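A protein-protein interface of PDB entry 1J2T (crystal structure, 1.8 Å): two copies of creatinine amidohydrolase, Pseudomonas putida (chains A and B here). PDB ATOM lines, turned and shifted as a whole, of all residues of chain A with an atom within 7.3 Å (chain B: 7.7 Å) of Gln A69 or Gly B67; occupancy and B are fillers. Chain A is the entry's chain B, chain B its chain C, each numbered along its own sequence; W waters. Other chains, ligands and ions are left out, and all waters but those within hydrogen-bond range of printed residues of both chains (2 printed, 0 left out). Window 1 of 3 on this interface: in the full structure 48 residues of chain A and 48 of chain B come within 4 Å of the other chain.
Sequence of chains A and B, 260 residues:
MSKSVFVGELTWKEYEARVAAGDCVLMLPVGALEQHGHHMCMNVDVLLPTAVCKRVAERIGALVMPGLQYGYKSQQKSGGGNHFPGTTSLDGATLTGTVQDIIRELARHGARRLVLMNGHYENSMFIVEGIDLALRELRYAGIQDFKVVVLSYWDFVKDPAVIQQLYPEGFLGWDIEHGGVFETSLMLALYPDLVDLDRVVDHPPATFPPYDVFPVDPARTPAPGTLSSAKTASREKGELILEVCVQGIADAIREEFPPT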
ATOM      1  N   PRO A  29      35.636  15.861  17.577  1.00  0.00           N
ATOM      2  CA  PRO A  29      36.053  14.642  16.884  1.00  0.00           C
ATOM      3  C   PRO A  29      35.009  14.241  15.841  1.00  0.00           C
ATOM      4  O   PRO A  29      33.798  14.325  16.110  1.00  0.00           O
ATOM      5  CB  PRO A  29      36.130  13.596  18.004  1.00  0.00           C
ATOM      6  CG  PRO A  29      35.904  14.318  19.283  1.00  0.00           C
ATOM      7  CD  PRO A  29      35.234  15.607  18.970  1.00  0.00           C
ATOM      8  N   VAL A  30      35.461  13.835  14.660  1.00  0.00           N
ATOM      9  CA  VAL A  30      34.555  13.412  13.597  1.00  0.00           C
ATOM     10  C   VAL A  30      34.963  12.032  13.102  1.00  0.00           C
ATOM     11  O   VAL A  30      35.989  11.880  12.429  1.00  0.00           O
ATOM     12  CB  VAL A  30      34.547  14.404  12.415  1.00  0.00           C
ATOM     13  CG1 VAL A  30      33.500  14.013  11.408  1.00  0.00           C
ATOM     14  CG2 VAL A  30      34.279  15.807  12.907  1.00  0.00           C
ATOM     15  N   GLY A  31      34.156  11.025  13.421  1.00  0.00           N
ATOM     16  CA  GLY A  31      34.494   9.667  13.066  1.00  0.00           C
ATOM     17  C   GLY A  31      33.587   8.961  12.094  1.00  0.00           C
ATOM     18  O   GLY A  31      33.137   9.520  11.086  1.00  0.00           O
ATOM     19  N   ALA A  32      33.332   7.694  12.411  1.00  0.00           N
ATOM     20  CA  ALA A  32      32.570   6.804  11.571  1.00  0.00           C
ATOM     21  C   ALA A  32      32.293   5.492  12.327  1.00  0.00           C
ATOM     22  O   ALA A  32      32.960   5.187  13.316  1.00  0.00           O
ATOM     23  CB  ALA A  32      33.343   6.493  10.291  1.00  0.00           C
ATOM     24  N   LEU A  33      31.298   4.755  11.850  1.00  0.00           N
ATOM     25  CA  LEU A  33      31.023   3.385  12.283  1.00  0.00           C
ATOM     26  C   LEU A  33      31.349   2.591  11.038  1.00  0.00           C
ATOM     27  O   LEU A  33      30.640   2.645  10.028  1.00  0.00           O
ATOM     28  CB  LEU A  33      29.576   3.178  12.703  1.00  0.00           C
ATOM     29  CG  LEU A  33      29.272   1.750  13.177  1.00  0.00           C
ATOM     30  CD1 LEU A  33      30.063   1.429  14.441  1.00  0.00           C
ATOM     31  CD2 LEU A  33      27.785   1.582  13.433  1.00  0.00           C
ATOM     32  N   GLU A  34      32.449   1.854  11.094  1.00  0.00           N
ATOM     33  CA  GLU A  34      32.960   1.229   9.897  1.00  0.00           C
ATOM     34  C   GLU A  34      33.732  -0.032  10.215  1.00  0.00           C
ATOM     35  O   GLU A  34      34.443  -0.081  11.214  1.00  0.00           O
ATOM     36  CB  GLU A  34      33.902   2.225   9.212  1.00  0.00           C
ATOM     37  CG  GLU A  34      34.522   1.779   7.896  1.00  0.00           C
ATOM     38  CD  GLU A  34      35.562   2.763   7.390  1.00  0.00           C
ATOM     39  OE1 GLU A  34      35.598   2.989   6.165  1.00  0.00           O
ATOM     40  OE2 GLU A  34      36.347   3.309   8.208  1.00  0.00           O
ATOM     41  N   MET A  42      34.376  -1.753  15.317  1.00  0.00           N
ATOM     42  CA  MET A  42      33.940  -0.831  14.261  1.00  0.00           C
ATOM     43  C   MET A  42      33.899   0.655  14.634  1.00  0.00           C
ATOM     44  O   MET A  42      33.684   1.491  13.744  1.00  0.00           O
ATOM     45  CB  MET A  42      32.573  -1.268  13.731  1.00  0.00           C
ATOM     46  CG  MET A  42      32.626  -2.605  12.977  1.00  0.00           C
ATOM     47  SD  MET A  42      31.184  -3.054  12.093  1.00  0.00           S
ATOM     48  CE  MET A  42      30.100  -3.512  13.489  1.00  0.00           C
ATOM     49  N   ASN A  43      34.122   1.006  15.902  1.00  0.00           N
ATOM     50  CA  ASN A  43      34.082   2.420  16.308  1.00  0.00           C
ATOM     51  C   ASN A  43      35.449   3.107  16.395  1.00  0.00           C
ATOM     52  O   ASN A  43      35.580   4.189  16.962  1.00  0.00           O
ATOM     53  CB  ASN A  43      33.290   2.609  17.621  1.00  0.00           C
ATOM     54  CG  ASN A  43      33.954   1.944  18.815  1.00  0.00           C
ATOM     55  OD1 ASN A  43      33.356   1.841  19.906  1.00  0.00           O
ATOM     56  ND2 ASN A  43      35.176   1.474  18.623  1.00  0.00           N
ATOM     57  N   ASP A  45      37.255   4.838  14.329  1.00  0.00           N
ATOM     58  CA  ASP A  45      37.362   6.199  13.798  1.00  0.00           C
ATOM     59  C   ASP A  45      36.787   7.266  14.727  1.00  0.00           C
ATOM     60  O   ASP A  45      37.086   8.445  14.565  1.00  0.00           O
ATOM     61  CB  ASP A  45      36.728   6.279  12.416  1.00  0.00           C
ATOM     62  CG  ASP A  45      37.538   5.566  11.360  1.00  0.00           C
ATOM     63  OD1 ASP A  45      38.590   4.972  11.706  1.00  0.00           O
ATOM     64  OD2 ASP A  45      37.201   5.555  10.165  1.00  0.00           O
ATOM     65  N   VAL A  46      35.968   6.851  15.695  1.00  0.00           N
ATOM     66  CA  VAL A  46      35.509   7.760  16.748  1.00  0.00           C
ATOM     67  C   VAL A  46      36.476   7.688  17.920  1.00  0.00           C
ATOM     68  O   VAL A  46      36.960   8.702  18.394  1.00  0.00           O
ATOM     69  CB  VAL A  46      34.083   7.422  17.258  1.00  0.00           C
ATOM     70  CG1 VAL A  46      33.685   8.345  18.408  1.00  0.00           C
ATOM     71  CG2 VAL A  46      33.089   7.525  16.139  1.00  0.00           C
ATOM     72  N   LEU A  47      36.755   6.480  18.390  1.00  0.00           N
ATOM     73  CA  LEU A  47      37.621   6.312  19.555  1.00  0.00           C
ATOM     74  C   LEU A  47      38.958   7.019  19.435  1.00  0.00           C
ATOM     75  O   LEU A  47      39.395   7.697  20.363  1.00  0.00           O
ATOM     76  CB  LEU A  47      37.884   4.826  19.818  1.00  0.00           C
ATOM     77  CG  LEU A  47      36.736   3.987  20.386  1.00  0.00           C
ATOM     78  CD1 LEU A  47      37.224   2.558  20.608  1.00  0.00           C
ATOM     79  CD2 LEU A  47      36.179   4.570  21.677  1.00  0.00           C
ATOM     80  N   THR A  50      38.927  10.921  19.395  1.00  0.00           N
ATOM     81  CA  THR A  50      38.420  11.348  20.692  1.00  0.00           C
ATOM     82  C   THR A  50      39.514  11.254  21.765  1.00  0.00           C
ATOM     83  O   THR A  50      39.670  12.163  22.575  1.00  0.00           O
ATOM     84  CB  THR A  50      37.177  10.529  21.082  1.00  0.00           C
ATOM     85  OG1 THR A  50      36.139  10.717  20.093  1.00  0.00           O
ATOM     86  CG2 THR A  50      36.572  11.033  22.409  1.00  0.00           C
ATOM     87  N   PRO A  66      30.989  16.451  22.067  1.00  0.00           N
ATOM     88  CA  PRO A  66      30.569  15.092  21.716  1.00  0.00           C
ATOM     89  C   PRO A  66      30.927  14.787  20.265  1.00  0.00           C
ATOM     90  O   PRO A  66      30.705  15.612  19.364  1.00  0.00           O
ATOM     91  CB  PRO A  66      29.054  15.122  21.953  1.00  0.00           C
ATOM     92  CG  PRO A  66      28.877  16.178  23.015  1.00  0.00           C
ATOM     93  CD  PRO A  66      29.894  17.224  22.676  1.00  0.00           C
ATOM     94  N   GLY A  67      31.492  13.613  20.035  1.00  0.00           N
ATOM     95  CA  GLY A  67      31.976  13.287  18.711  1.00  0.00           C
ATOM     96  C   GLY A  67      30.890  12.920  17.724  1.00  0.00           C
ATOM     97  O   GLY A  67      29.792  12.463  18.102  1.00  0.00           O
ATOM     98  N   LEU A  68      31.177  13.149  16.444  1.00  0.00           N
ATOM     99  CA  LEU A  68      30.296  12.674  15.396  1.00  0.00           C
ATOM    100  C   LEU A  68      30.588  11.192  15.210  1.00  0.00           C
ATOM    101  O   LEU A  68      31.717  10.800  14.903  1.00  0.00           O
ATOM    102  CB  LEU A  68      30.468  13.472  14.108  1.00  0.00           C
ATOM    103  CG  LEU A  68      30.243  14.981  14.255  1.00  0.00           C
ATOM    104  CD1 LEU A  68      30.135  15.634  12.885  1.00  0.00           C
ATOM    105  CD2 LEU A  68      29.019  15.294  15.074  1.00  0.00           C
ATOM    106  N   GLN A  69      29.555  10.375  15.419  1.00  0.00           N
ATOM    107  CA  GLN A  69      29.668   8.923  15.461  1.00  0.00           C
ATOM    108  C   GLN A  69      29.532   8.253  14.099  1.00  0.00           C
ATOM    109  O   GLN A  69      29.965   7.098  13.922  1.00  0.00           O
ATOM    110  CB  GLN A  69      28.566   8.351  16.363  1.00  0.00           C
ATOM    111  CG  GLN A  69      28.391   9.060  17.699  1.00  0.00           C
ATOM    112  CD  GLN A  69      29.491   8.751  18.687  1.00  0.00           C
ATOM    113  OE1 GLN A  69      29.744   7.586  19.003  1.00  0.00           O
ATOM    114  NE2 GLN A  69      30.121   9.793  19.212  1.00  0.00           N
ATOM    115  N   TYR A  70      28.880   8.946  13.167  1.00  0.00           N
ATOM    116  CA  TYR A  70      28.621   8.416  11.844  1.00  0.00           C
ATOM    117  C   TYR A  70      29.243   9.354  10.826  1.00  0.00           C
ATOM    118  O   TYR A  70      29.067  10.573  10.916  1.00  0.00           O
ATOM    119  CB  TYR A  70      27.121   8.281  11.599  1.00  0.00           C
ATOM    120  CG  TYR A  70      26.429   7.337  12.572  1.00  0.00           C
ATOM    121  CD1 TYR A  70      25.923   7.795  13.774  1.00  0.00           C
ATOM    122  CD2 TYR A  70      26.272   5.991  12.267  1.00  0.00           C
ATOM    123  CE1 TYR A  70      25.297   6.925  14.665  1.00  0.00           C
ATOM    124  CE2 TYR A  70      25.647   5.130  13.133  1.00  0.00           C
ATOM    125  CZ  TYR A  70      25.158   5.594  14.326  1.00  0.00           C
ATOM    126  OH  TYR A  70      24.533   4.721  15.205  1.00  0.00           O
ATOM    127  N   GLY A  71      29.949   8.786   9.858  1.00  0.00           N
ATOM    128  CA  GLY A  71      30.639   9.560   8.843  1.00  0.00           C
ATOM    129  C   GLY A  71      30.204   9.229   7.431  1.00  0.00           C
ATOM    130  O   GLY A  71      29.241   8.490   7.203  1.00  0.00           O
ATOM    131  N   THR A  88      28.062   1.960   8.744  1.00  0.00           N
ATOM    132  CA  THR A  88      26.800   2.660   8.714  1.00  0.00           C
ATOM    133  C   THR A  88      27.097   4.113   8.408  1.00  0.00           C
ATOM    134  O   THR A  88      27.555   4.851   9.280  1.00  0.00           O
ATOM    135  CB  THR A  88      26.147   2.533  10.089  1.00  0.00           C
ATOM    136  OG1 THR A  88      25.967   1.137  10.404  1.00  0.00           O
ATOM    137  CG2 THR A  88      24.753   3.138  10.081  1.00  0.00           C
ATOM    138  N   LEU A  90      26.510   8.080   6.555  1.00  0.00           N
ATOM    139  CA  LEU A  90      25.617   9.177   6.234  1.00  0.00           C
ATOM    140  C   LEU A  90      25.794   9.635   4.792  1.00  0.00           C
ATOM    141  O   LEU A  90      26.861   9.461   4.185  1.00  0.00           O
ATOM    142  CB  LEU A  90      25.913  10.367   7.145  1.00  0.00           C
ATOM    143  CG  LEU A  90      25.853  10.129   8.655  1.00  0.00           C
ATOM    144  CD1 LEU A  90      26.104  11.435   9.379  1.00  0.00           C
ATOM    145  CD2 LEU A  90      24.510   9.527   9.038  1.00  0.00           C
ATOM    146  N   PHE B   6      27.282  -3.502  22.366  1.00  0.00           N
ATOM    147  CA  PHE B   6      27.462  -2.331  21.494  1.00  0.00           C
ATOM    148  C   PHE B   6      28.041  -2.688  20.129  1.00  0.00           C
ATOM    149  O   PHE B   6      29.132  -3.260  20.017  1.00  0.00           O
ATOM    150  CB  PHE B   6      28.342  -1.291  22.180  1.00  0.00           C
ATOM    151  CG  PHE B   6      27.715  -0.669  23.378  1.00  0.00           C
ATOM    152  CD1 PHE B   6      28.075  -1.077  24.652  1.00  0.00           C
ATOM    153  CD2 PHE B   6      26.737   0.318  23.241  1.00  0.00           C
ATOM    154  CE1 PHE B   6      27.491  -0.510  25.768  1.00  0.00           C
ATOM    155  CE2 PHE B   6      26.160   0.888  24.352  1.00  0.00           C
ATOM    156  CZ  PHE B   6      26.536   0.471  25.620  1.00  0.00           C
ATOM    157  N   MET B  27      19.104  -1.325  18.569  1.00  0.00           N
ATOM    158  CA  MET B  27      18.595  -0.215  19.361  1.00  0.00           C
ATOM    159  C   MET B  27      19.454   1.037  19.123  1.00  0.00           C
ATOM    160  O   MET B  27      20.684   0.957  19.110  1.00  0.00           O
ATOM    161  CB  MET B  27      18.569  -0.611  20.849  1.00  0.00           C
ATOM    162  CG  MET B  27      17.904  -1.984  21.063  1.00  0.00           C
ATOM    163  SD  MET B  27      18.075  -2.716  22.699  1.00  0.00           S
ATOM    164  CE  MET B  27      17.271  -1.495  23.704  1.00  0.00           C
ATOM    165  N   LEU B  28      18.800   2.177  18.913  1.00  0.00           N
ATOM    166  CA  LEU B  28      19.495   3.438  18.670  1.00  0.00           C
ATOM    167  C   LEU B  28      19.080   4.509  19.675  1.00  0.00           C
ATOM    168  O   LEU B  28      17.935   4.987  19.642  1.00  0.00           O
ATOM    169  CB  LEU B  28      19.217   3.917  17.242  1.00  0.00           C
ATOM    170  CG  LEU B  28      19.771   5.310  16.872  1.00  0.00           C
ATOM    171  CD1 LEU B  28      21.272   5.298  17.015  1.00  0.00           C
ATOM    172  CD2 LEU B  28      19.369   5.703  15.447  1.00  0.00           C
ATOM    173  N   PRO B  29      19.984   4.890  20.566  1.00  0.00           N
ATOM    174  CA  PRO B  29      19.716   5.979  21.505  1.00  0.00           C
ATOM    175  C   PRO B  29      19.758   7.325  20.769  1.00  0.00           C
ATOM    176  O   PRO B  29      20.649   7.535  19.944  1.00  0.00           O
ATOM    177  CB  PRO B  29      20.871   5.872  22.515  1.00  0.00           C
ATOM    178  CG  PRO B  29      21.579   4.600  22.189  1.00  0.00           C
ATOM    179  CD  PRO B  29      21.318   4.299  20.781  1.00  0.00           C
ATOM    180  N   VAL B  30      18.786   8.194  21.019  1.00  0.00           N
ATOM    181  CA  VAL B  30      18.754   9.507  20.376  1.00  0.00           C
ATOM    182  C   VAL B  30      18.665  10.569  21.455  1.00  0.00           C
ATOM    183  O   VAL B  30      17.647  10.702  22.135  1.00  0.00           O
ATOM    184  CB  VAL B  30      17.564   9.641  19.417  1.00  0.00           C
ATOM    185  CG1 VAL B  30      17.664  10.932  18.635  1.00  0.00           C
ATOM    186  CG2 VAL B  30      17.508   8.465  18.470  1.00  0.00           C
ATOM    187  N   GLY B  31      19.743  11.324  21.622  1.00  0.00           N
ATOM    188  CA  GLY B  31      19.826  12.283  22.697  1.00  0.00           C
ATOM    189  C   GLY B  31      19.938  13.728  22.282  1.00  0.00           C
ATOM    190  O   GLY B  31      19.260  14.183  21.354  1.00  0.00           O
ATOM    191  N   VAL B  46      21.850  11.804  26.239  1.00  0.00           N
ATOM    192  CA  VAL B  46      22.527  10.711  25.570  1.00  0.00           C
ATOM    193  C   VAL B  46      22.808   9.611  26.603  1.00  0.00           C
ATOM    194  O   VAL B  46      22.498   8.447  26.383  1.00  0.00           O
ATOM    195  CB  VAL B  46      23.866  11.163  24.943  1.00  0.00           C
ATOM    196  CG1 VAL B  46      24.617   9.959  24.358  1.00  0.00           C
ATOM    197  CG2 VAL B  46      23.613  12.207  23.878  1.00  0.00           C
ATOM    198  N   THR B  50      21.187   5.637  26.586  1.00  0.00           N
ATOM    199  CA  THR B  50      22.258   4.698  26.261  1.00  0.00           C
ATOM    200  C   THR B  50      22.387   3.628  27.348  1.00  0.00           C
ATOM    201  O   THR B  50      22.497   2.439  27.046  1.00  0.00           O
ATOM    202  CB  THR B  50      23.574   5.444  26.054  1.00  0.00           C
ATOM    203  OG1 THR B  50      23.454   6.308  24.907  1.00  0.00           O
ATOM    204  CG2 THR B  50      24.701   4.469  25.697  1.00  0.00           C
ATOM    205  N   VAL B  64      23.256  -2.497  20.463  1.00  0.00           N
ATOM    206  CA  VAL B  64      23.036  -1.055  20.577  1.00  0.00           C
ATOM    207  C   VAL B  64      23.961  -0.278  19.643  1.00  0.00           C
ATOM    208  O   VAL B  64      25.180  -0.455  19.670  1.00  0.00           O
ATOM    209  CB  VAL B  64      23.281  -0.572  22.013  1.00  0.00           C
ATOM    210  CG1 VAL B  64      22.900   0.893  22.180  1.00  0.00           C
ATOM    211  CG2 VAL B  64      22.513  -1.450  23.011  1.00  0.00           C
ATOM    212  N   MET B  65      23.363   0.569  18.811  1.00  0.00           N
ATOM    213  CA  MET B  65      24.118   1.387  17.852  1.00  0.00           C
ATOM    214  C   MET B  65      24.689   2.619  18.547  1.00  0.00           C
ATOM    215  O   MET B  65      24.185   3.027  19.601  1.00  0.00           O
ATOM    216  CB  MET B  65      23.181   1.852  16.734  1.00  0.00           C
ATOM    217  CG  MET B  65      22.685   0.752  15.810  1.00  0.00           C
ATOM    218  SD  MET B  65      23.927   0.103  14.710  1.00  0.00           S
ATOM    219  CE  MET B  65      24.149   1.517  13.556  1.00  0.00           C
ATOM    220  N   PRO B  66      25.733   3.236  17.976  1.00  0.00           N
ATOM    221  CA  PRO B  66      26.231   4.506  18.510  1.00  0.00           C
ATOM    222  C   PRO B  66      25.108   5.551  18.591  1.00  0.00           C
ATOM    223  O   PRO B  66      24.311   5.696  17.664  1.00  0.00           O
ATOM    224  CB  PRO B  66      27.311   4.918  17.509  1.00  0.00           C
ATOM    225  CG  PRO B  66      27.786   3.647  16.934  1.00  0.00           C
ATOM    226  CD  PRO B  66      26.545   2.762  16.844  1.00  0.00           C
ATOM    227  N   GLY B  67      25.056   6.282  19.693  1.00  0.00           N
ATOM    228  CA  GLY B  67      23.960   7.202  19.915  1.00  0.00           C
ATOM    229  C   GLY B  67      24.063   8.511  19.155  1.00  0.00           C
ATOM    230  O   GLY B  67      25.152   8.961  18.769  1.00  0.00           O
ATOM    231  N   LEU B  68      22.904   9.110  18.914  1.00  0.00           N
ATOM    232  CA  LEU B  68      22.865  10.427  18.309  1.00  0.00           C
ATOM    233  C   LEU B  68      23.110  11.400  19.456  1.00  0.00           C
ATOM    234  O   LEU B  68      22.369  11.440  20.437  1.00  0.00           O
ATOM    235  CB  LEU B  68      21.535  10.646  17.588  1.00  0.00           C
ATOM    236  CG  LEU B  68      21.197   9.655  16.462  1.00  0.00           C
ATOM    237  CD1 LEU B  68      20.061  10.207  15.591  1.00  0.00           C
ATOM    238  CD2 LEU B  68      22.407   9.353  15.607  1.00  0.00           C
ATOM    239  N   GLN B  69      24.197  12.149  19.344  1.00  0.00           N
ATOM    240  CA  GLN B  69      24.695  13.030  20.398  1.00  0.00           C
ATOM    241  C   GLN B  69      24.055  14.413  20.399  1.00  0.00           C
ATOM    242  O   GLN B  69      24.038  15.102  21.432  1.00  0.00           O
ATOM    243  CB  GLN B  69      26.203  13.203  20.214  1.00  0.00           C
ATOM    244  CG  GLN B  69      26.962  11.899  19.962  1.00  0.00           C
ATOM    245  CD  GLN B  69      27.139  11.046  21.205  1.00  0.00           C
ATOM    246  OE1 GLN B  69      27.679  11.509  22.210  1.00  0.00           O
ATOM    247  NE2 GLN B  69      26.724   9.776  21.126  1.00  0.00           N
ATOM    248  N   TYR B  70      23.569  14.824  19.238  1.00  0.00           N
ATOM    249  CA  TYR B  70      22.951  16.127  19.057  1.00  0.00           C
ATOM    250  C   TYR B  70      21.528  15.933  18.574  1.00  0.00           C
ATOM    251  O   TYR B  70      21.279  15.146  17.653  1.00  0.00           O
ATOM    252  CB  TYR B  70      23.745  16.939  18.036  1.00  0.00           C
ATOM    253  CG  TYR B  70      25.193  17.146  18.427  1.00  0.00           C
ATOM    254  CD1 TYR B  70      26.181  16.249  18.037  1.00  0.00           C
ATOM    255  CD2 TYR B  70      25.579  18.254  19.182  1.00  0.00           C
ATOM    256  CE1 TYR B  70      27.529  16.449  18.406  1.00  0.00           C
ATOM    257  CE2 TYR B  70      26.907  18.455  19.549  1.00  0.00           C
ATOM    258  CZ  TYR B  70      27.879  17.546  19.162  1.00  0.00           C
ATOM    259  OH  TYR B  70      29.208  17.770  19.522  1.00  0.00           O
ATOM    260  N   THR B  98      19.569  12.177   9.450  1.00  0.00           N
ATOM    261  CA  THR B  98      20.474  11.274  10.151  1.00  0.00           C
ATOM    262  C   THR B  98      19.765   9.946  10.441  1.00  0.00           C
ATOM    263  O   THR B  98      20.297   8.859  10.187  1.00  0.00           O
ATOM    264  CB  THR B  98      20.973  11.930  11.431  1.00  0.00           C
ATOM    265  OG1 THR B  98      21.713  13.124  11.104  1.00  0.00           O
ATOM    266  CG2 THR B  98      21.969  11.057  12.154  1.00  0.00           C
ATOM    267  N   ILE B 102      20.589   6.233   8.682  1.00  0.00           N
ATOM    268  CA  ILE B 102      20.938   5.080   9.501  1.00  0.00           C
ATOM    269  C   ILE B 102      19.989   3.920   9.196  1.00  0.00           C
ATOM    270  O   ILE B 102      20.437   2.790   9.034  1.00  0.00           O
ATOM    271  CB  ILE B 102      20.953   5.446  10.984  1.00  0.00           C
ATOM    272  CG1 ILE B 102      22.168   6.319  11.279  1.00  0.00           C
ATOM    273  CG2 ILE B 102      21.019   4.209  11.844  1.00  0.00           C
ATOM    274  CD1 ILE B 102      22.137   7.003  12.625  1.00  0.00           C
HETATM  275  O   HOH W   1      30.488  11.741  22.334  1.00  0.00           O
HETATM  276  O   HOH W   2      28.043   6.245  20.854  1.00  0.00           O
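The backbone carbonyl oxygen of Pro A66 sits at hydrogen-bond distance from the side-chain hydroxyl of Tyr B70 (2.6 Å).
OH of Tyr A70 lies within hydrogen-bond range of O of Pro B66 (2.7 Å).
The backbone carbonyl oxygen of Met B27 is in hydrogen-bond range of the backbone NH of Met B65 (2.7 Å).
The backbone NH (N) of Gly A31 sits at hydrogen-bond distance from the backbone carbonyl oxygen (O) of Leu A68.
N of Gly B31 lies within hydrogen-bond range of O of Leu B68 (2.9 Å).
The backbone carbonyl oxygen (O) of Pro B29 lies within hydrogen-bond range of the backbone NH (N) of Leu B68 (2.9 Å).
The backbone NH (N) of Leu A33 sits at hydrogen-bond distance from the backbone carbonyl oxygen (O) of Gln A69 (3.4 Å).
NE2 of Gln A69 is in hydrogen-bond range of O of Gly A67.
Among the printed residues, pairs that only touch across the chains: Leu A33 with Met B65 (3.6 Å), Leu A33 with Pro B66 (3.8 Å), Pro A66 with Gln B69 (3.9 Å), Gly A67 with Gln B69 (3.4 Å), Leu A68 with Tyr B70 (3.8 Å), Gln A69 with Pro B66 (3.8 Å), Gln A69 with Gly B67 (3.4 Å), Gln A69 with Gln B69 (3.8 Å), Tyr A70 with Leu B28 (3.8 Å), Tyr A70 with Met B65 (3.5 Å), Tyr A70 with Leu B68 (3.9 Å), Tyr A70 with Ile B102 (3.7 Å) and Thr A88 with Met B65 (3.7 Å).
Gln A69 touches just these residues of chain B: Pro B66 (3.8 Å), Gly B67 (3.4 Å) and Gln B69 (3.8 Å).
Of chain A, only Gln A69 (3.4 Å) comes within 4 Å of Gly B67.
Of the printed residues of chain A, Tyr B70 touches Pro A66 (2.6 Å) and Leu A68 (3.8 Å).
Of the printed residues of chain A, Met B65 touches Leu A33, Tyr A70 and Thr A88.
Of the printed residues of chain B, Leu A33 touches Met B65 (3.6 Å) and Pro B66 (3.8 Å).
Of the printed residues of chain A, Gln B69 touches Pro A66, Gly A67 and Gln A69.
Printed residues of chain A within 4 Å of Leu B68: Tyr A70.
Pro B29 touches none of the printed residues of chain A.
Val A46 touches none of the printed residues of chain B.
The nearest residue of chain B that does not touch Gln A69 is Leu B68 (5.6 Å).
The nearest printed residue of chain A that does not touch Pro B66 is Asn A43 (5.6 Å).
Of the 20 printed residues of chain A, 7 touch a printed residue of chain B.
Printed residues of chain A that touch a printed residue of chain B: Leu A33, Pro A66, Gly A67, Leu A68, Gln A69, Tyr A70 and Thr A88.
Along chain A the printed residues that touch a printed residue of chain B span positions 33 to 88.
Hydrophobic or aromatic side chains of chain B that line the printed part of chain A: Leu B28, Met B65, Pro B66, Leu B68, Tyr B70 and Ile B102.
Among the printed residues, no Asp or Glu carboxylate lies within 4 Å of a Lys or Arg side-chain nitrogen of the other chain.
Pro A66 touches Gln B69, and with the chains exchanged Gln A69 touches Pro B66.
Pro A66 touches Tyr B70, and with the chains exchanged Tyr A70 touches Pro B66.
Gly A67 touches Gln B69, and with the chains exchanged Gln A69 touches Gly B67.
Leu A68 touches Tyr B70, and with the chains exchanged Tyr A70 touches Leu B68.
Positions printed for both chains: 29, 30, 31, 46, 50, 66, 67, 68, 69 and 70.
Of the 15 pairs that touch across the chains among the printed residues, 9 have their exchanged pair printed and touching as well.
Water W1 lies within hydrogen-bond range of OE1 of Gln B69 (2.8 Å) and N of Gly A67 (3.1 Å).
Water W2 lies within hydrogen-bond range of the side-chain amide oxygen (OE1) of Gln A69 (2.8 Å) and the backbone NH (N) of Gly B67 (3.2 Å).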
